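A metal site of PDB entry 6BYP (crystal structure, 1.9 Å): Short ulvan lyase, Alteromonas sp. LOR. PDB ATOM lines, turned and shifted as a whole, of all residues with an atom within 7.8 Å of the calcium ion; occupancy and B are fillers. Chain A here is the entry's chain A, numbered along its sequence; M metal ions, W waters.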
ATOM      1  N   VAL A 169      30.127 -24.036 -10.442  1.00  0.00           N
ATOM      2  CA  VAL A 169      30.591 -24.914 -11.510  1.00  0.00           C
ATOM      3  C   VAL A 169      29.401 -25.296 -12.384  1.00  0.00           C
ATOM      4  O   VAL A 169      28.349 -25.726 -11.877  1.00  0.00           O
ATOM      5  CB  VAL A 169      31.280 -26.151 -10.912  1.00  0.00           C
ATOM      6  CG1 VAL A 169      31.504 -27.191 -11.990  1.00  0.00           C
ATOM      7  CG2 VAL A 169      32.603 -25.728 -10.254  1.00  0.00           C
ATOM      8  N   ASP A 170      29.547 -25.109 -13.693  1.00  0.00           N
ATOM      9  CA  ASP A 170      28.498 -25.396 -14.659  1.00  0.00           C
ATOM     10  C   ASP A 170      27.291 -24.482 -14.514  1.00  0.00           C
ATOM     11  O   ASP A 170      26.211 -24.803 -15.013  1.00  0.00           O
ATOM     12  CB  ASP A 170      28.029 -26.855 -14.550  1.00  0.00           C
ATOM     13  CG  ASP A 170      29.155 -27.842 -14.777  1.00  0.00           C
ATOM     14  OD1 ASP A 170      30.190 -27.432 -15.332  1.00  0.00           O
ATOM     15  OD2 ASP A 170      28.990 -29.018 -14.410  1.00  0.00           O
ATOM     16  N   ASP A 171      27.452 -23.331 -13.833  1.00  0.00           N
ATOM     17  CA  ASP A 171      26.300 -22.525 -13.466  1.00  0.00           C
ATOM     18  C   ASP A 171      26.736 -21.087 -13.200  1.00  0.00           C
ATOM     19  O   ASP A 171      26.096 -20.394 -12.403  1.00  0.00           O
ATOM     20  CB  ASP A 171      25.613 -23.137 -12.238  1.00  0.00           C
ATOM     21  CG  ASP A 171      24.228 -22.561 -11.976  1.00  0.00           C
ATOM     22  OD1 ASP A 171      23.486 -22.292 -12.953  1.00  0.00           O
ATOM     23  OD2 ASP A 171      23.873 -22.401 -10.783  1.00  0.00           O
ATOM     24  N   PHE A 173      26.895 -18.633 -15.553  1.00  0.00           N
ATOM     25  CA  PHE A 173      26.074 -17.758 -16.373  1.00  0.00           C
ATOM     26  C   PHE A 173      24.691 -18.375 -16.356  1.00  0.00           C
ATOM     27  O   PHE A 173      24.552 -19.567 -16.630  1.00  0.00           O
ATOM     28  CB  PHE A 173      26.628 -17.667 -17.805  1.00  0.00           C
ATOM     29  CG  PHE A 173      25.902 -16.675 -18.688  1.00  0.00           C
ATOM     30  CD1 PHE A 173      24.736 -17.031 -19.334  1.00  0.00           C
ATOM     31  CD2 PHE A 173      26.399 -15.386 -18.849  1.00  0.00           C
ATOM     32  CE1 PHE A 173      24.065 -16.107 -20.130  1.00  0.00           C
ATOM     33  CE2 PHE A 173      25.746 -14.470 -19.645  1.00  0.00           C
ATOM     34  CZ  PHE A 173      24.577 -14.834 -20.280  1.00  0.00           C
ATOM     35  N   ARG A 174      23.665 -17.582 -16.028  1.00  0.00           N
ATOM     36  CA  ARG A 174      22.344 -18.125 -15.688  1.00  0.00           C
ATOM     37  C   ARG A 174      21.302 -17.507 -16.619  1.00  0.00           C
ATOM     38  O   ARG A 174      20.891 -16.364 -16.415  1.00  0.00           O
ATOM     39  CB  ARG A 174      22.024 -17.882 -14.202  1.00  0.00           C
ATOM     40  CG  ARG A 174      23.006 -18.595 -13.271  1.00  0.00           C
ATOM     41  CD  ARG A 174      22.980 -18.067 -11.838  1.00  0.00           C
ATOM     42  NE  ARG A 174      23.564 -19.062 -10.933  1.00  0.00           N
ATOM     43  CZ  ARG A 174      23.744 -18.908  -9.633  1.00  0.00           C
ATOM     44  NH1 ARG A 174      23.407 -17.765  -9.038  1.00  0.00           N
ATOM     45  NH2 ARG A 174      24.236 -19.908  -8.918  1.00  0.00           N
ATOM     46  N   TYR A 175      20.876 -18.277 -17.620  1.00  0.00           N
ATOM     47  CA  TYR A 175      19.984 -17.801 -18.669  1.00  0.00           C
ATOM     48  C   TYR A 175      18.781 -18.723 -18.761  1.00  0.00           C
ATOM     49  O   TYR A 175      18.942 -19.939 -18.895  1.00  0.00           O
ATOM     50  CB  TYR A 175      20.741 -17.763 -20.007  1.00  0.00           C
ATOM     51  CG  TYR A 175      19.915 -17.509 -21.243  1.00  0.00           C
ATOM     52  CD1 TYR A 175      19.022 -16.456 -21.317  1.00  0.00           C
ATOM     53  CD2 TYR A 175      20.082 -18.323 -22.365  1.00  0.00           C
ATOM     54  CE1 TYR A 175      18.284 -16.221 -22.492  1.00  0.00           C
ATOM     55  CE2 TYR A 175      19.372 -18.099 -23.529  1.00  0.00           C
ATOM     56  CZ  TYR A 175      18.466 -17.050 -23.592  1.00  0.00           C
ATOM     57  OH  TYR A 175      17.753 -16.857 -24.753  1.00  0.00           O
ATOM     58  N   LYS A 197      13.960 -26.232 -20.488  1.00  0.00           N
ATOM     59  CA  LYS A 197      14.875 -26.814 -19.519  1.00  0.00           C
ATOM     60  C   LYS A 197      16.267 -26.983 -20.117  1.00  0.00           C
ATOM     61  O   LYS A 197      16.429 -27.140 -21.328  1.00  0.00           O
ATOM     62  CB  LYS A 197      14.366 -28.182 -19.028  1.00  0.00           C
ATOM     63  CG  LYS A 197      13.141 -28.082 -18.133  1.00  0.00           C
ATOM     64  CD  LYS A 197      12.913 -29.372 -17.350  1.00  0.00           C
ATOM     65  CE  LYS A 197      11.551 -29.360 -16.676  1.00  0.00           C
ATOM     66  NZ  LYS A 197      11.208 -30.718 -16.167  1.00  0.00           N
ATOM     67  N   ASP A 198      17.271 -26.970 -19.242  1.00  0.00           N
ATOM     68  CA  ASP A 198      18.637 -27.362 -19.584  1.00  0.00           C
ATOM     69  C   ASP A 198      18.680 -28.882 -19.665  1.00  0.00           C
ATOM     70  O   ASP A 198      18.528 -29.580 -18.654  1.00  0.00           O
ATOM     71  CB  ASP A 198      19.596 -26.841 -18.521  1.00  0.00           C
ATOM     72  CG  ASP A 198      21.057 -27.232 -18.794  1.00  0.00           C
ATOM     73  OD1 ASP A 198      21.333 -27.906 -19.811  1.00  0.00           O
ATOM     74  OD2 ASP A 198      21.917 -26.839 -17.978  1.00  0.00           O
ATOM     75  N   THR A 199      18.831 -29.405 -20.878  1.00  0.00           N
ATOM     76  CA  THR A 199      18.979 -30.843 -21.099  1.00  0.00           C
ATOM     77  C   THR A 199      20.361 -31.189 -21.657  1.00  0.00           C
ATOM     78  O   THR A 199      20.517 -32.249 -22.280  1.00  0.00           O
ATOM     79  CB  THR A 199      17.880 -31.377 -22.018  1.00  0.00           C
ATOM     80  OG1 THR A 199      17.831 -30.606 -23.226  1.00  0.00           O
ATOM     81  CG2 THR A 199      16.515 -31.318 -21.329  1.00  0.00           C
ATOM     82  N   SER A 200      21.350 -30.326 -21.435  1.00  0.00           N
ATOM     83  CA  SER A 200      22.697 -30.542 -21.937  1.00  0.00           C
ATOM     84  C   SER A 200      23.443 -31.543 -21.063  1.00  0.00           C
ATOM     85  O   SER A 200      22.977 -31.973 -20.008  1.00  0.00           O
ATOM     86  CB  SER A 200      23.469 -29.233 -21.962  1.00  0.00           C
ATOM     87  OG  SER A 200      23.808 -28.827 -20.640  1.00  0.00           O
ATOM     88  N   LEU A 202      25.626 -30.895 -19.129  1.00  0.00           N
ATOM     89  CA  LEU A 202      25.908 -30.261 -17.841  1.00  0.00           C
ATOM     90  C   LEU A 202      24.657 -29.996 -17.024  1.00  0.00           C
ATOM     91  O   LEU A 202      24.743 -29.360 -15.966  1.00  0.00           O
ATOM     92  CB  LEU A 202      26.682 -28.961 -18.036  1.00  0.00           C
ATOM     93  CG  LEU A 202      28.016 -29.098 -18.757  1.00  0.00           C
ATOM     94  CD1 LEU A 202      28.684 -27.731 -18.848  1.00  0.00           C
ATOM     95  CD2 LEU A 202      28.902 -30.085 -18.017  1.00  0.00           C
ATOM     96  N   SER A 203      23.488 -30.450 -17.479  1.00  0.00           N
ATOM     97  CA  SER A 203      22.254 -30.254 -16.734  1.00  0.00           C
ATOM     98  C   SER A 203      22.403 -30.737 -15.297  1.00  0.00           C
ATOM     99  O   SER A 203      22.946 -31.809 -15.047  1.00  0.00           O
ATOM    100  CB  SER A 203      21.097 -31.010 -17.408  1.00  0.00           C
ATOM    101  OG  SER A 203      19.930 -30.937 -16.632  1.00  0.00           O
ATOM    102  N   GLN A 204      21.864 -29.972 -14.357  1.00  0.00           N
ATOM    103  CA  GLN A 204      21.921 -30.343 -12.951  1.00  0.00           C
ATOM    104  C   GLN A 204      20.718 -31.139 -12.484  1.00  0.00           C
ATOM    105  O   GLN A 204      20.715 -31.623 -11.346  1.00  0.00           O
ATOM    106  CB  GLN A 204      22.089 -29.106 -12.058  1.00  0.00           C
ATOM    107  CG  GLN A 204      23.357 -28.320 -12.373  1.00  0.00           C
ATOM    108  CD  GLN A 204      23.521 -27.095 -11.499  1.00  0.00           C
ATOM    109  OE1 GLN A 204      22.643 -26.230 -11.442  1.00  0.00           O
ATOM    110  NE2 GLN A 204      24.653 -27.024 -10.802  1.00  0.00           N
ATOM    111  N   GLY A 205      19.704 -31.331 -13.340  1.00  0.00           N
ATOM    112  CA  GLY A 205      18.573 -32.146 -12.972  1.00  0.00           C
ATOM    113  C   GLY A 205      17.295 -31.710 -13.681  1.00  0.00           C
ATOM    114  O   GLY A 205      17.315 -30.820 -14.530  1.00  0.00           O
ATOM    115  N   ASP A 207      14.771 -30.035 -12.720  1.00  0.00           N
ATOM    116  CA  ASP A 207      14.268 -28.695 -12.456  1.00  0.00           C
ATOM    117  C   ASP A 207      15.263 -27.609 -12.861  1.00  0.00           C
ATOM    118  O   ASP A 207      15.163 -26.480 -12.387  1.00  0.00           O
ATOM    119  CB  ASP A 207      13.881 -28.535 -10.981  1.00  0.00           C
ATOM    120  CG  ASP A 207      15.067 -28.678 -10.041  1.00  0.00           C
ATOM    121  OD1 ASP A 207      16.099 -29.253 -10.452  1.00  0.00           O
ATOM    122  OD2 ASP A 207      14.944 -28.248  -8.879  1.00  0.00           O
ATOM    123  N   ASP A 208      16.233 -27.954 -13.698  1.00  0.00           N
ATOM    124  CA  ASP A 208      17.285 -27.048 -14.135  1.00  0.00           C
ATOM    125  C   ASP A 208      16.788 -26.288 -15.358  1.00  0.00           C
ATOM    126  O   ASP A 208      16.720 -26.859 -16.453  1.00  0.00           O
ATOM    127  CB  ASP A 208      18.558 -27.843 -14.434  1.00  0.00           C
ATOM    128  CG  ASP A 208      19.725 -26.977 -14.898  1.00  0.00           C
ATOM    129  OD1 ASP A 208      19.571 -25.746 -15.087  1.00  0.00           O
ATOM    130  OD2 ASP A 208      20.811 -27.561 -15.077  1.00  0.00           O
ATOM    131  N   TYR A 209      16.445 -25.011 -15.168  1.00  0.00           N
ATOM    132  CA  TYR A 209      16.035 -24.107 -16.236  1.00  0.00           C
ATOM    133  C   TYR A 209      17.117 -23.097 -16.604  1.00  0.00           C
ATOM    134  O   TYR A 209      16.839 -22.133 -17.327  1.00  0.00           O
ATOM    135  CB  TYR A 209      14.766 -23.343 -15.813  1.00  0.00           C
ATOM    136  CG  TYR A 209      13.488 -24.159 -15.907  1.00  0.00           C
ATOM    137  CD1 TYR A 209      13.075 -24.959 -14.843  1.00  0.00           C
ATOM    138  CD2 TYR A 209      12.692 -24.113 -17.041  1.00  0.00           C
ATOM    139  CE1 TYR A 209      11.905 -25.699 -14.935  1.00  0.00           C
ATOM    140  CE2 TYR A 209      11.530 -24.857 -17.133  1.00  0.00           C
ATOM    141  CZ  TYR A 209      11.134 -25.644 -16.091  1.00  0.00           C
ATOM    142  OH  TYR A 209       9.971 -26.368 -16.205  1.00  0.00           O
ATOM    143  N   LYS A 210      18.340 -23.292 -16.101  1.00  0.00           N
ATOM    144  CA  LYS A 210      19.414 -22.314 -16.294  1.00  0.00           C
ATOM    145  C   LYS A 210      20.359 -22.818 -17.376  1.00  0.00           C
ATOM    146  O   LYS A 210      20.949 -23.889 -17.237  1.00  0.00           O
ATOM    147  CB  LYS A 210      20.184 -22.070 -15.000  1.00  0.00           C
ATOM    148  CG  LYS A 210      19.395 -21.350 -13.933  1.00  0.00           C
ATOM    149  CD  LYS A 210      20.151 -21.294 -12.618  1.00  0.00           C
ATOM    150  CE  LYS A 210      20.180 -22.683 -11.958  1.00  0.00           C
ATOM    151  NZ  LYS A 210      20.891 -22.685 -10.656  1.00  0.00           N
ATOM    152  N   HIS A 211      20.543 -22.019 -18.427  1.00  0.00           N
ATOM    153  CA  HIS A 211      21.459 -22.357 -19.506  1.00  0.00           C
ATOM    154  C   HIS A 211      22.764 -21.598 -19.326  1.00  0.00           C
ATOM    155  O   HIS A 211      22.775 -20.420 -18.968  1.00  0.00           O
ATOM    156  CB  HIS A 211      20.815 -22.039 -20.851  1.00  0.00           C
ATOM    157  CG  HIS A 211      19.583 -22.836 -21.098  1.00  0.00           C
ATOM    158  ND1 HIS A 211      19.556 -23.938 -21.916  1.00  0.00           N
ATOM    159  CD2 HIS A 211      18.350 -22.759 -20.542  1.00  0.00           C
ATOM    160  CE1 HIS A 211      18.350 -24.467 -21.910  1.00  0.00           C
ATOM    161  NE2 HIS A 211      17.599 -23.778 -21.071  1.00  0.00           N
ATOM    162  N   LEU A 212      23.870 -22.298 -19.593  1.00  0.00           N
ATOM    163  CA  LEU A 212      25.200 -21.760 -19.340  1.00  0.00           C
ATOM    164  C   LEU A 212      25.680 -20.829 -20.448  1.00  0.00           C
ATOM    165  O   LEU A 212      26.607 -20.037 -20.219  1.00  0.00           O
ATOM    166  CB  LEU A 212      26.176 -22.943 -19.152  1.00  0.00           C
ATOM    167  CG  LEU A 212      27.550 -22.586 -18.589  1.00  0.00           C
ATOM    168  CD1 LEU A 212      27.396 -21.852 -17.257  1.00  0.00           C
ATOM    169  CD2 LEU A 212      28.408 -23.820 -18.425  1.00  0.00           C
HETATM  170 CA    CA M   1      22.043 -25.633 -15.945  1.00  0.00          CA
HETATM  171  O   HOH W   1      23.936 -24.156 -16.611  1.00  0.00           O
HETATM  172  O   HOH W   2      22.481 -24.650 -13.750  1.00  0.00           O
HETATM  173  O   HOH W   3      24.039 -26.908 -15.375  1.00  0.00           O
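Water W2 bridges the side-chain carboxylate (OD1) of Asp 171 (2.7 Å) and the side-chain amide oxygen (OE1) of Gln 204 (2.8 Å). Water W3 bridges the backbone carbonyl oxygen (O) of Leu 202 and the backbone carbonyl oxygen (O) of Asp 170.
OD2 of Asp 208 lies close to N of Gln 204. The side-chain carboxylate (OD1) of Asp 198 sits at hydrogen-bond distance from the side-chain hydroxyl (OG) of Ser 200, 2.8 Å away. The backbone carbonyl oxygen of Asp 198 lies within hydrogen-bond range of the side-chain hydroxyl of Ser 203, at 2.8 Å. The side-chain carboxylate (OD2) of Asp 171 is in salt-bridge range of the side-chain amino group (NZ) of Lys 210 (3.0 Å).
The calcium ion is bound by the side-chain carboxylate (OD2) of Asp 198, the backbone carbonyl oxygen (O) of Lys 210, water W3, water W2, the side-chain carboxylate (OD2) of Asp 208, water W1 and the side-chain carboxylate (OD1) of Asp 208. The calcium ion has seven donor atoms within binding distance.
The nearest printed residue that does not touch the calcium ion is Asp 170 (4.4 Å).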
